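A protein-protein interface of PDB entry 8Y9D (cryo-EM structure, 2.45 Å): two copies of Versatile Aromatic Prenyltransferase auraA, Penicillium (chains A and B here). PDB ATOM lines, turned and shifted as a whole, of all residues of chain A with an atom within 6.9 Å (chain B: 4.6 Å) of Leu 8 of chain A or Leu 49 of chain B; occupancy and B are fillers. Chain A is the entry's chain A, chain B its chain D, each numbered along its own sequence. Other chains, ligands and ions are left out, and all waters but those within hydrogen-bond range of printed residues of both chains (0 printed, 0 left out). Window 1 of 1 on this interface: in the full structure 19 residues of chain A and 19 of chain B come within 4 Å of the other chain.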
ATOM      1  N   SER A   3      -7.854 -32.209 -11.527  1.00  0.00           N
ATOM      2  CA  SER A   3      -8.865 -31.874 -10.547  1.00  0.00           C
ATOM      3  C   SER A   3      -9.081 -30.371 -10.508  1.00  0.00           C
ATOM      4  O   SER A   3      -8.206 -29.595 -10.897  1.00  0.00           O
ATOM      5  CB  SER A   3      -8.450 -32.382  -9.178  1.00  0.00           C
ATOM      6  OG  SER A   3      -7.356 -31.641  -8.680  1.00  0.00           O
ATOM      7  N   PRO A   4     -10.250 -29.928 -10.052  1.00  0.00           N
ATOM      8  CA  PRO A   4     -10.527 -28.487 -10.043  1.00  0.00           C
ATOM      9  C   PRO A   4      -9.471 -27.663  -9.339  1.00  0.00           C
ATOM     10  O   PRO A   4      -9.134 -26.577  -9.820  1.00  0.00           O
ATOM     11  CB  PRO A   4     -11.882 -28.411  -9.336  1.00  0.00           C
ATOM     12  CG  PRO A   4     -12.501 -29.687  -9.583  1.00  0.00           C
ATOM     13  CD  PRO A   4     -11.431 -30.707  -9.660  1.00  0.00           C
ATOM     14  N   TRP A   5      -8.922 -28.147  -8.226  1.00  0.00           N
ATOM     15  CA  TRP A   5      -7.955 -27.349  -7.485  1.00  0.00           C
ATOM     16  C   TRP A   5      -6.617 -27.279  -8.203  1.00  0.00           C
ATOM     17  O   TRP A   5      -6.000 -26.212  -8.247  1.00  0.00           O
ATOM     18  CB  TRP A   5      -7.796 -27.888  -6.060  1.00  0.00           C
ATOM     19  CG  TRP A   5      -7.579 -29.356  -5.903  1.00  0.00           C
ATOM     20  CD1 TRP A   5      -6.393 -29.986  -5.696  1.00  0.00           C
ATOM     21  CD2 TRP A   5      -8.577 -30.377  -5.897  1.00  0.00           C
ATOM     22  NE1 TRP A   5      -6.584 -31.328  -5.578  1.00  0.00           N
ATOM     23  CE2 TRP A   5      -7.919 -31.598  -5.697  1.00  0.00           C
ATOM     24  CE3 TRP A   5      -9.963 -30.380  -6.054  1.00  0.00           C
ATOM     25  CZ2 TRP A   5      -8.593 -32.806  -5.651  1.00  0.00           C
ATOM     26  CZ3 TRP A   5     -10.627 -31.579  -6.010  1.00  0.00           C
ATOM     27  CH2 TRP A   5      -9.943 -32.776  -5.810  1.00  0.00           C
ATOM     28  N   ASP A   6      -6.172 -28.379  -8.806  1.00  0.00           N
ATOM     29  CA  ASP A   6      -4.953 -28.346  -9.606  1.00  0.00           C
ATOM     30  C   ASP A   6      -5.084 -27.368 -10.769  1.00  0.00           C
ATOM     31  O   ASP A   6      -4.270 -26.447 -10.922  1.00  0.00           O
ATOM     32  CB  ASP A   6      -4.635 -29.751 -10.109  1.00  0.00           C
ATOM     33  CG  ASP A   6      -4.207 -30.683  -9.001  1.00  0.00           C
ATOM     34  OD1 ASP A   6      -3.499 -30.230  -8.080  1.00  0.00           O
ATOM     35  OD2 ASP A   6      -4.579 -31.875  -9.049  1.00  0.00           O
ATOM     36  N   PHE A   7      -6.103 -27.562 -11.605  1.00  0.00           N
ATOM     37  CA  PHE A   7      -6.299 -26.702 -12.763  1.00  0.00           C
ATOM     38  C   PHE A   7      -6.467 -25.244 -12.353  1.00  0.00           C
ATOM     39  O   PHE A   7      -5.928 -24.340 -12.998  1.00  0.00           O
ATOM     40  CB  PHE A   7      -7.508 -27.189 -13.564  1.00  0.00           C
ATOM     41  CG  PHE A   7      -7.901 -26.270 -14.668  1.00  0.00           C
ATOM     42  CD1 PHE A   7      -7.134 -26.170 -15.809  1.00  0.00           C
ATOM     43  CD2 PHE A   7      -9.032 -25.494 -14.563  1.00  0.00           C
ATOM     44  CE1 PHE A   7      -7.491 -25.322 -16.816  1.00  0.00           C
ATOM     45  CE2 PHE A   7      -9.389 -24.649 -15.570  1.00  0.00           C
ATOM     46  CZ  PHE A   7      -8.617 -24.564 -16.698  1.00  0.00           C
ATOM     47  N   LEU A   8      -7.213 -24.994 -11.279  1.00  0.00           N
ATOM     48  CA  LEU A   8      -7.455 -23.623 -10.850  1.00  0.00           C
ATOM     49  C   LEU A   8      -6.180 -22.970 -10.342  1.00  0.00           C
ATOM     50  O   LEU A   8      -5.887 -21.820 -10.680  1.00  0.00           O
ATOM     51  CB  LEU A   8      -8.538 -23.598  -9.782  1.00  0.00           C
ATOM     52  CG  LEU A   8      -9.980 -23.641 -10.261  1.00  0.00           C
ATOM     53  CD1 LEU A   8     -10.878 -23.878  -9.093  1.00  0.00           C
ATOM     54  CD2 LEU A   8     -10.354 -22.369 -10.982  1.00  0.00           C
ATOM     55  N   GLY A   9      -5.407 -23.681  -9.526  1.00  0.00           N
ATOM     56  CA  GLY A   9      -4.117 -23.162  -9.125  1.00  0.00           C
ATOM     57  C   GLY A   9      -3.219 -22.884 -10.306  1.00  0.00           C
ATOM     58  O   GLY A   9      -2.375 -21.985 -10.255  1.00  0.00           O
ATOM     59  N   ARG A  10      -3.382 -23.651 -11.381  1.00  0.00           N
ATOM     60  CA  ARG A  10      -2.636 -23.380 -12.602  1.00  0.00           C
ATOM     61  C   ARG A  10      -3.103 -22.088 -13.264  1.00  0.00           C
ATOM     62  O   ARG A  10      -2.283 -21.283 -13.718  1.00  0.00           O
ATOM     63  CB  ARG A  10      -2.771 -24.561 -13.558  1.00  0.00           C
ATOM     64  CG  ARG A  10      -1.945 -25.761 -13.168  1.00  0.00           C
ATOM     65  CD  ARG A  10      -1.456 -26.528 -14.364  1.00  0.00           C
ATOM     66  NE  ARG A  10      -2.461 -27.440 -14.885  1.00  0.00           N
ATOM     67  CZ  ARG A  10      -2.817 -28.566 -14.284  1.00  0.00           C
ATOM     68  NH1 ARG A  10      -2.263 -28.912 -13.135  1.00  0.00           N
ATOM     69  NH2 ARG A  10      -3.734 -29.343 -14.830  1.00  0.00           N
ATOM     70  N   VAL A  11      -4.415 -21.865 -13.321  1.00  0.00           N
ATOM     71  CA  VAL A  11      -4.934 -20.714 -14.053  1.00  0.00           C
ATOM     72  C   VAL A  11      -5.153 -19.493 -13.165  1.00  0.00           C
ATOM     73  O   VAL A  11      -4.996 -18.361 -13.629  1.00  0.00           O
ATOM     74  CB  VAL A  11      -6.234 -21.069 -14.797  1.00  0.00           C
ATOM     75  CG1 VAL A  11      -5.977 -22.119 -15.819  1.00  0.00           C
ATOM     76  CG2 VAL A  11      -7.314 -21.518 -13.851  1.00  0.00           C
ATOM     77  N   LEU A  12      -5.514 -19.686 -11.904  1.00  0.00           N
ATOM     78  CA  LEU A  12      -5.953 -18.565 -11.089  1.00  0.00           C
ATOM     79  C   LEU A  12      -4.826 -17.571 -10.867  1.00  0.00           C
ATOM     80  O   LEU A  12      -3.668 -17.944 -10.670  1.00  0.00           O
ATOM     81  CB  LEU A  12      -6.488 -19.056  -9.748  1.00  0.00           C
ATOM     82  CG  LEU A  12      -7.845 -19.742  -9.776  1.00  0.00           C
ATOM     83  CD1 LEU A  12      -8.269 -20.120  -8.376  1.00  0.00           C
ATOM     84  CD2 LEU A  12      -8.857 -18.863 -10.443  1.00  0.00           C
ATOM     85  N   GLN A  13      -5.182 -16.296 -10.908  1.00  0.00           N
ATOM     86  CA  GLN A  13      -4.272 -15.204 -10.606  1.00  0.00           C
ATOM     87  C   GLN A  13      -4.559 -14.753  -9.182  1.00  0.00           C
ATOM     88  O   GLN A  13      -5.703 -14.441  -8.841  1.00  0.00           O
ATOM     89  CB  GLN A  13      -4.443 -14.059 -11.599  1.00  0.00           C
ATOM     90  CG  GLN A  13      -3.969 -14.362 -13.006  1.00  0.00           C
ATOM     91  CD  GLN A  13      -2.475 -14.516 -13.096  1.00  0.00           C
ATOM     92  OE1 GLN A  13      -1.965 -15.589 -13.413  1.00  0.00           O
ATOM     93  NE2 GLN A  13      -1.760 -13.440 -12.820  1.00  0.00           N
ATOM     94  N   PHE A  14      -3.525 -14.736  -8.352  1.00  0.00           N
ATOM     95  CA  PHE A  14      -3.674 -14.431  -6.941  1.00  0.00           C
ATOM     96  C   PHE A  14      -3.140 -13.044  -6.629  1.00  0.00           C
ATOM     97  O   PHE A  14      -2.086 -12.644  -7.127  1.00  0.00           O
ATOM     98  CB  PHE A  14      -2.957 -15.475  -6.091  1.00  0.00           C
ATOM     99  CG  PHE A  14      -3.538 -16.851  -6.206  1.00  0.00           C
ATOM    100  CD1 PHE A  14      -3.124 -17.706  -7.199  1.00  0.00           C
ATOM    101  CD2 PHE A  14      -4.497 -17.285  -5.325  1.00  0.00           C
ATOM    102  CE1 PHE A  14      -3.653 -18.960  -7.307  1.00  0.00           C
ATOM    103  CE2 PHE A  14      -5.025 -18.542  -5.433  1.00  0.00           C
ATOM    104  CZ  PHE A  14      -4.601 -19.379  -6.427  1.00  0.00           C
ATOM    105  N   LYS A  20      -1.828 -17.563  -2.469  1.00  0.00           N
ATOM    106  CA  LYS A  20      -1.367 -18.720  -3.224  1.00  0.00           C
ATOM    107  C   LYS A  20      -0.921 -19.850  -2.304  1.00  0.00           C
ATOM    108  O   LYS A  20      -1.194 -21.024  -2.573  1.00  0.00           O
ATOM    109  CB  LYS A  20      -0.230 -18.283  -4.142  1.00  0.00           C
ATOM    110  CG  LYS A  20       0.374 -19.372  -4.988  1.00  0.00           C
ATOM    111  CD  LYS A  20      -0.666 -20.200  -5.670  1.00  0.00           C
ATOM    112  CE  LYS A  20      -0.057 -21.076  -6.723  1.00  0.00           C
ATOM    113  NZ  LYS A  20      -0.818 -22.321  -6.888  1.00  0.00           N
ATOM    114  N   TRP A  23      -3.862 -21.372  -0.671  1.00  0.00           N
ATOM    115  CA  TRP A  23      -4.489 -22.209  -1.680  1.00  0.00           C
ATOM    116  C   TRP A  23      -3.790 -23.553  -1.786  1.00  0.00           C
ATOM    117  O   TRP A  23      -4.431 -24.604  -1.711  1.00  0.00           O
ATOM    118  CB  TRP A  23      -4.478 -21.491  -3.025  1.00  0.00           C
ATOM    119  CG  TRP A  23      -5.094 -22.290  -4.103  1.00  0.00           C
ATOM    120  CD1 TRP A  23      -4.465 -23.149  -4.940  1.00  0.00           C
ATOM    121  CD2 TRP A  23      -6.476 -22.330  -4.454  1.00  0.00           C
ATOM    122  NE1 TRP A  23      -5.359 -23.722  -5.789  1.00  0.00           N
ATOM    123  CE2 TRP A  23      -6.606 -23.235  -5.513  1.00  0.00           C
ATOM    124  CE3 TRP A  23      -7.616 -21.689  -3.976  1.00  0.00           C
ATOM    125  CZ2 TRP A  23      -7.823 -23.514  -6.103  1.00  0.00           C
ATOM    126  CZ3 TRP A  23      -8.814 -21.967  -4.562  1.00  0.00           C
ATOM    127  CH2 TRP A  23      -8.913 -22.870  -5.614  1.00  0.00           C
ATOM    128  N   GLN A  44     -17.685 -28.057  -6.991  1.00  0.00           N
ATOM    129  CA  GLN A  44     -16.306 -27.934  -6.538  1.00  0.00           C
ATOM    130  C   GLN A  44     -15.668 -26.664  -7.069  1.00  0.00           C
ATOM    131  O   GLN A  44     -15.005 -25.935  -6.326  1.00  0.00           O
ATOM    132  CB  GLN A  44     -15.500 -29.151  -6.968  1.00  0.00           C
ATOM    133  CG  GLN A  44     -15.886 -30.414  -6.273  1.00  0.00           C
ATOM    134  CD  GLN A  44     -15.162 -31.616  -6.807  1.00  0.00           C
ATOM    135  OE1 GLN A  44     -13.941 -31.620  -6.926  1.00  0.00           O
ATOM    136  NE2 GLN A  44     -15.913 -32.647  -7.135  1.00  0.00           N
ATOM    137  N   TYR A  45     -15.839 -26.391  -8.361  1.00  0.00           N
ATOM    138  CA  TYR A  45     -15.299 -25.167  -8.940  1.00  0.00           C
ATOM    139  C   TYR A  45     -15.871 -23.940  -8.249  1.00  0.00           C
ATOM    140  O   TYR A  45     -15.132 -23.029  -7.866  1.00  0.00           O
ATOM    141  CB  TYR A  45     -15.589 -25.125 -10.441  1.00  0.00           C
ATOM    142  CG  TYR A  45     -14.572 -25.835 -11.293  1.00  0.00           C
ATOM    143  CD1 TYR A  45     -13.355 -25.251 -11.581  1.00  0.00           C
ATOM    144  CD2 TYR A  45     -14.832 -27.084 -11.814  1.00  0.00           C
ATOM    145  CE1 TYR A  45     -12.428 -25.896 -12.355  1.00  0.00           C
ATOM    146  CE2 TYR A  45     -13.913 -27.731 -12.585  1.00  0.00           C
ATOM    147  CZ  TYR A  45     -12.712 -27.134 -12.856  1.00  0.00           C
ATOM    148  OH  TYR A  45     -11.788 -27.782 -13.626  1.00  0.00           O
ATOM    149  N   ARG A  46     -17.192 -23.904  -8.074  1.00  0.00           N
ATOM    150  CA  ARG A  46     -17.820 -22.741  -7.458  1.00  0.00           C
ATOM    151  C   ARG A  46     -17.324 -22.519  -6.033  1.00  0.00           C
ATOM    152  O   ARG A  46     -17.012 -21.388  -5.644  1.00  0.00           O
ATOM    153  CB  ARG A  46     -19.334 -22.903  -7.491  1.00  0.00           C
ATOM    154  CG  ARG A  46     -19.932 -22.468  -8.792  1.00  0.00           C
ATOM    155  CD  ARG A  46     -21.421 -22.612  -8.819  1.00  0.00           C
ATOM    156  NE  ARG A  46     -22.072 -21.720  -7.871  1.00  0.00           N
ATOM    157  CZ  ARG A  46     -23.384 -21.541  -7.820  1.00  0.00           C
ATOM    158  NH1 ARG A  46     -24.168 -22.179  -8.669  1.00  0.00           N
ATOM    159  NH2 ARG A  46     -23.908 -20.719  -6.927  1.00  0.00           N
ATOM    160  N   LEU A  48     -14.491 -23.710  -4.575  1.00  0.00           N
ATOM    161  CA  LEU A  48     -13.081 -23.366  -4.564  1.00  0.00           C
ATOM    162  C   LEU A  48     -12.853 -21.936  -5.019  1.00  0.00           C
ATOM    163  O   LEU A  48     -11.927 -21.277  -4.544  1.00  0.00           O
ATOM    164  CB  LEU A  48     -12.317 -24.348  -5.438  1.00  0.00           C
ATOM    165  CG  LEU A  48     -12.148 -25.738  -4.841  1.00  0.00           C
ATOM    166  CD1 LEU A  48     -11.746 -26.712  -5.901  1.00  0.00           C
ATOM    167  CD2 LEU A  48     -11.137 -25.722  -3.726  1.00  0.00           C
ATOM    168  N   LEU A  49     -13.703 -21.420  -5.899  1.00  0.00           N
ATOM    169  CA  LEU A  49     -13.589 -20.025  -6.296  1.00  0.00           C
ATOM    170  C   LEU A  49     -14.113 -19.083  -5.224  1.00  0.00           C
ATOM    171  O   LEU A  49     -13.628 -17.956  -5.110  1.00  0.00           O
ATOM    172  CB  LEU A  49     -14.326 -19.802  -7.613  1.00  0.00           C
ATOM    173  CG  LEU A  49     -13.647 -20.447  -8.817  1.00  0.00           C
ATOM    174  CD1 LEU A  49     -14.623 -20.692  -9.939  1.00  0.00           C
ATOM    175  CD2 LEU A  49     -12.476 -19.612  -9.275  1.00  0.00           C
ATOM    176  N   TYR A  52     -11.220 -18.944  -3.008  1.00  0.00           N
ATOM    177  CA  TYR A  52     -10.190 -18.108  -3.615  1.00  0.00           C
ATOM    178  C   TYR A  52     -10.529 -16.626  -3.518  1.00  0.00           C
ATOM    179  O   TYR A  52      -9.641 -15.792  -3.321  1.00  0.00           O
ATOM    180  CB  TYR A  52      -9.999 -18.546  -5.069  1.00  0.00           C
ATOM    181  CG  TYR A  52      -9.519 -17.501  -6.046  1.00  0.00           C
ATOM    182  CD1 TYR A  52      -8.182 -17.173  -6.141  1.00  0.00           C
ATOM    183  CD2 TYR A  52     -10.398 -16.877  -6.908  1.00  0.00           C
ATOM    184  CE1 TYR A  52      -7.746 -16.239  -7.039  1.00  0.00           C
ATOM    185  CE2 TYR A  52      -9.967 -15.946  -7.803  1.00  0.00           C
ATOM    186  CZ  TYR A  52      -8.640 -15.630  -7.866  1.00  0.00           C
ATOM    187  OH  TYR A  52      -8.191 -14.699  -8.759  1.00  0.00           O
ATOM    188  N   LEU B   8     -17.727 -16.374 -12.710  1.00  0.00           N
ATOM    189  CA  LEU B   8     -16.287 -16.237 -12.867  1.00  0.00           C
ATOM    190  C   LEU B   8     -15.883 -14.777 -12.994  1.00  0.00           C
ATOM    191  O   LEU B   8     -14.913 -14.338 -12.369  1.00  0.00           O
ATOM    192  CB  LEU B   8     -15.817 -17.035 -14.074  1.00  0.00           C
ATOM    193  CG  LEU B   8     -15.594 -18.524 -13.871  1.00  0.00           C
ATOM    194  CD1 LEU B   8     -15.403 -19.176 -15.200  1.00  0.00           C
ATOM    195  CD2 LEU B   8     -14.413 -18.781 -12.967  1.00  0.00           C
ATOM    196  N   LEU B  12     -13.176 -13.816 -10.667  1.00  0.00           N
ATOM    197  CA  LEU B  12     -11.860 -13.832 -11.282  1.00  0.00           C
ATOM    198  C   LEU B  12     -11.143 -12.507 -11.087  1.00  0.00           C
ATOM    199  O   LEU B  12     -11.744 -11.433 -11.156  1.00  0.00           O
ATOM    200  CB  LEU B  12     -11.968 -14.151 -12.769  1.00  0.00           C
ATOM    201  CG  LEU B  12     -12.301 -15.592 -13.125  1.00  0.00           C
ATOM    202  CD1 LEU B  12     -12.318 -15.770 -14.625  1.00  0.00           C
ATOM    203  CD2 LEU B  12     -11.332 -16.525 -12.468  1.00  0.00           C
ATOM    204  N   TYR B  45     -16.480 -24.264 -17.302  1.00  0.00           N
ATOM    205  CA  TYR B  45     -15.542 -23.626 -16.387  1.00  0.00           C
ATOM    206  C   TYR B  45     -14.114 -23.775 -16.884  1.00  0.00           C
ATOM    207  O   TYR B  45     -13.354 -22.802 -16.927  1.00  0.00           O
ATOM    208  CB  TYR B  45     -15.690 -24.220 -14.985  1.00  0.00           C
ATOM    209  CG  TYR B  45     -16.759 -23.576 -14.146  1.00  0.00           C
ATOM    210  CD1 TYR B  45     -16.544 -22.359 -13.533  1.00  0.00           C
ATOM    211  CD2 TYR B  45     -17.980 -24.190 -13.961  1.00  0.00           C
ATOM    212  CE1 TYR B  45     -17.517 -21.771 -12.770  1.00  0.00           C
ATOM    213  CE2 TYR B  45     -18.952 -23.611 -13.201  1.00  0.00           C
ATOM    214  CZ  TYR B  45     -18.717 -22.402 -12.605  1.00  0.00           C
ATOM    215  OH  TYR B  45     -19.693 -21.816 -11.846  1.00  0.00           O
ATOM    216  N   ARG B  46     -13.730 -24.991 -17.271  1.00  0.00           N
ATOM    217  CA  ARG B  46     -12.361 -25.223 -17.719  1.00  0.00           C
ATOM    218  C   ARG B  46     -12.024 -24.396 -18.955  1.00  0.00           C
ATOM    219  O   ARG B  46     -10.951 -23.785 -19.030  1.00  0.00           O
ATOM    220  CB  ARG B  46     -12.157 -26.709 -17.984  1.00  0.00           C
ATOM    221  CG  ARG B  46     -11.821 -27.474 -16.742  1.00  0.00           C
ATOM    222  CD  ARG B  46     -11.604 -28.932 -17.004  1.00  0.00           C
ATOM    223  NE  ARG B  46     -10.433 -29.168 -17.833  1.00  0.00           N
ATOM    224  CZ  ARG B  46      -9.936 -30.374 -18.071  1.00  0.00           C
ATOM    225  NH1 ARG B  46     -10.504 -31.436 -17.528  1.00  0.00           N
ATOM    226  NH2 ARG B  46      -8.871 -30.515 -18.841  1.00  0.00           N
ATOM    227  N   HIS B  47     -12.930 -24.350 -19.927  1.00  0.00           N
ATOM    228  CA  HIS B  47     -12.673 -23.625 -21.161  1.00  0.00           C
ATOM    229  C   HIS B  47     -12.685 -22.118 -20.956  1.00  0.00           C
ATOM    230  O   HIS B  47     -11.877 -21.402 -21.553  1.00  0.00           O
ATOM    231  CB  HIS B  47     -13.697 -24.031 -22.210  1.00  0.00           C
ATOM    232  CG  HIS B  47     -13.436 -25.371 -22.811  1.00  0.00           C
ATOM    233  ND1 HIS B  47     -12.165 -25.862 -22.996  1.00  0.00           N
ATOM    234  CD2 HIS B  47     -14.279 -26.329 -23.258  1.00  0.00           C
ATOM    235  CE1 HIS B  47     -12.235 -27.061 -23.538  1.00  0.00           C
ATOM    236  NE2 HIS B  47     -13.507 -27.369 -23.705  1.00  0.00           N
ATOM    237  N   LEU B  48     -13.594 -21.614 -20.127  1.00  0.00           N
ATOM    238  CA  LEU B  48     -13.602 -20.196 -19.819  1.00  0.00           C
ATOM    239  C   LEU B  48     -12.370 -19.787 -19.033  1.00  0.00           C
ATOM    240  O   LEU B  48     -11.882 -18.668 -19.189  1.00  0.00           O
ATOM    241  CB  LEU B  48     -14.875 -19.854 -19.061  1.00  0.00           C
ATOM    242  CG  LEU B  48     -16.140 -19.844 -19.907  1.00  0.00           C
ATOM    243  CD1 LEU B  48     -17.351 -19.887 -19.031  1.00  0.00           C
ATOM    244  CD2 LEU B  48     -16.178 -18.633 -20.801  1.00  0.00           C
ATOM    245  N   LEU B  49     -11.824 -20.687 -18.222  1.00  0.00           N
ATOM    246  CA  LEU B  49     -10.587 -20.382 -17.519  1.00  0.00           C
ATOM    247  C   LEU B  49      -9.377 -20.460 -18.435  1.00  0.00           C
ATOM    248  O   LEU B  49      -8.397 -19.743 -18.218  1.00  0.00           O
ATOM    249  CB  LEU B  49     -10.424 -21.326 -16.332  1.00  0.00           C
ATOM    250  CG  LEU B  49     -11.410 -21.068 -15.198  1.00  0.00           C
ATOM    251  CD1 LEU B  49     -11.601 -22.294 -14.342  1.00  0.00           C
ATOM    252  CD2 LEU B  49     -10.974 -19.880 -14.376  1.00  0.00           C
ATOM    253  N   VAL B  50      -9.418 -21.323 -19.447  1.00  0.00           N
ATOM    254  CA  VAL B  50      -8.418 -21.269 -20.510  1.00  0.00           C
ATOM    255  C   VAL B  50      -8.477 -19.918 -21.212  1.00  0.00           C
ATOM    256  O   VAL B  50      -7.454 -19.253 -21.415  1.00  0.00           O
ATOM    257  CB  VAL B  50      -8.633 -22.427 -21.500  1.00  0.00           C
ATOM    258  CG1 VAL B  50      -7.816 -22.243 -22.736  1.00  0.00           C
ATOM    259  CG2 VAL B  50      -8.284 -23.732 -20.864  1.00  0.00           C
ATOM    260  N   LEU B  51      -9.677 -19.508 -21.612  1.00  0.00           N
ATOM    261  CA  LEU B  51      -9.865 -18.203 -22.232  1.00  0.00           C
ATOM    262  C   LEU B  51      -9.333 -17.083 -21.345  1.00  0.00           C
ATOM    263  O   LEU B  51      -8.732 -16.123 -21.833  1.00  0.00           O
ATOM    264  CB  LEU B  51     -11.348 -18.010 -22.547  1.00  0.00           C
ATOM    265  CG  LEU B  51     -11.812 -16.617 -22.966  1.00  0.00           C
ATOM    266  CD1 LEU B  51     -11.403 -16.300 -24.385  1.00  0.00           C
ATOM    267  CD2 LEU B  51     -13.299 -16.492 -22.803  1.00  0.00           C
ATOM    268  N   TYR B  52      -9.560 -17.188 -20.037  1.00  0.00           N
ATOM    269  CA  TYR B  52      -9.114 -16.167 -19.095  1.00  0.00           C
ATOM    270  C   TYR B  52      -7.600 -16.171 -18.924  1.00  0.00           C
ATOM    271  O   TYR B  52      -6.984 -15.110 -18.781  1.00  0.00           O
ATOM    272  CB  TYR B  52      -9.829 -16.388 -17.760  1.00  0.00           C
ATOM    273  CG  TYR B  52      -9.114 -15.930 -16.512  1.00  0.00           C
ATOM    274  CD1 TYR B  52      -9.140 -14.607 -16.120  1.00  0.00           C
ATOM    275  CD2 TYR B  52      -8.456 -16.831 -15.700  1.00  0.00           C
ATOM    276  CE1 TYR B  52      -8.507 -14.197 -14.979  1.00  0.00           C
ATOM    277  CE2 TYR B  52      -7.825 -16.424 -14.564  1.00  0.00           C
ATOM    278  CZ  TYR B  52      -7.853 -15.106 -14.206  1.00  0.00           C
ATOM    279  OH  TYR B  52      -7.226 -14.683 -13.069  1.00  0.00           O
ATOM    280  N   ASP B  53      -6.981 -17.347 -18.949  1.00  0.00           N
ATOM    281  CA  ASP B  53      -5.572 -17.487 -18.615  1.00  0.00           C
ATOM    282  C   ASP B  53      -4.661 -17.382 -19.830  1.00  0.00           C
ATOM    283  O   ASP B  53      -3.643 -16.685 -19.787  1.00  0.00           O
ATOM    284  CB  ASP B  53      -5.336 -18.828 -17.923  1.00  0.00           C
ATOM    285  CG  ASP B  53      -3.937 -18.961 -17.377  1.00  0.00           C
ATOM    286  OD1 ASP B  53      -3.509 -18.076 -16.603  1.00  0.00           O
ATOM    287  OD2 ASP B  53      -3.261 -19.952 -17.723  1.00  0.00           O
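The backbone NH of Gln 13 of chain A lies close to the side-chain hydroxyl of Tyr 52 of chain B, at 3.4 Å. The backbone carbonyl oxygen (O) of Val 11 of chain A lies close to the side-chain carboxylate (OD1) of Asp 53 of chain B, 3.3 Å away.
The backbone carbonyl oxygen (O) of Gln 13 of chain A sits at hydrogen-bond distance from the side-chain hydroxyl (OH) of Tyr 52 of chain A, 2.5 Å away.
Among the printed residues, merely in contact across the chains: Tyr 45 of chain A with Arg 46 of chain B (3.1 Å), Arg 46 of chain A with Tyr 45 of chain B (3.1 Å), Phe 7 of chain A with Arg 46 of chain B (3.4 Å), Phe 7 of chain A with Leu 49 of chain B (3.5 Å), Val 11 of chain A with Tyr 52 of chain B (3.6 Å), Leu 8 of chain A with Leu 49 of chain B (3.6 Å), Leu 49 of chain A with Leu 8 of chain B (3.6 Å), Leu 12 of chain A with Leu 12 of chain B (3.96 Å) and Val 11 of chain A with Leu 49 of chain B (3.98 Å).
Leu 8 of chain A touches just one residue of chain B: Leu 49. Of the printed residues of chain B, Leu 12 of chain A touches Leu 12. Of the printed residues of chain B, Leu 49 of chain A touches Leu 8 (3.6 Å). Of the printed residues of chain A, Leu 49 of chain B touches Phe 7, Leu 8 and Val 11. Val 50 of chain B touches none of the printed residues of chain A. The nearest printed residue of chain A that does not touch Leu 49 of chain B is Tyr 45 of chain A (4.2 Å).
Of the 20 printed residues of chain A, 8 touch a printed residue of chain B. Hydrophobic or aromatic side chains of chain B that line the printed part of chain A: Leu 8, Leu 12, Tyr 45, Leu 49 and Tyr 52. Among the printed residues, 11 pairs touch across the chains. Among the printed residues, no Asp or Glu carboxylate lies within 4 Å of a Lys or Arg side-chain nitrogen of the other chain.
Leu 8 of chain A touches Leu 49 of chain B, and with the chains exchanged Leu 49 of chain A touches Leu 8 of chain B. Leu 12 of chain B touches its own counterpart, Leu 12 of chain A. Tyr 45 of chain A touches Arg 46 of chain B, and with the chains exchanged Arg 46 of chain A touches Tyr 45 of chain B.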
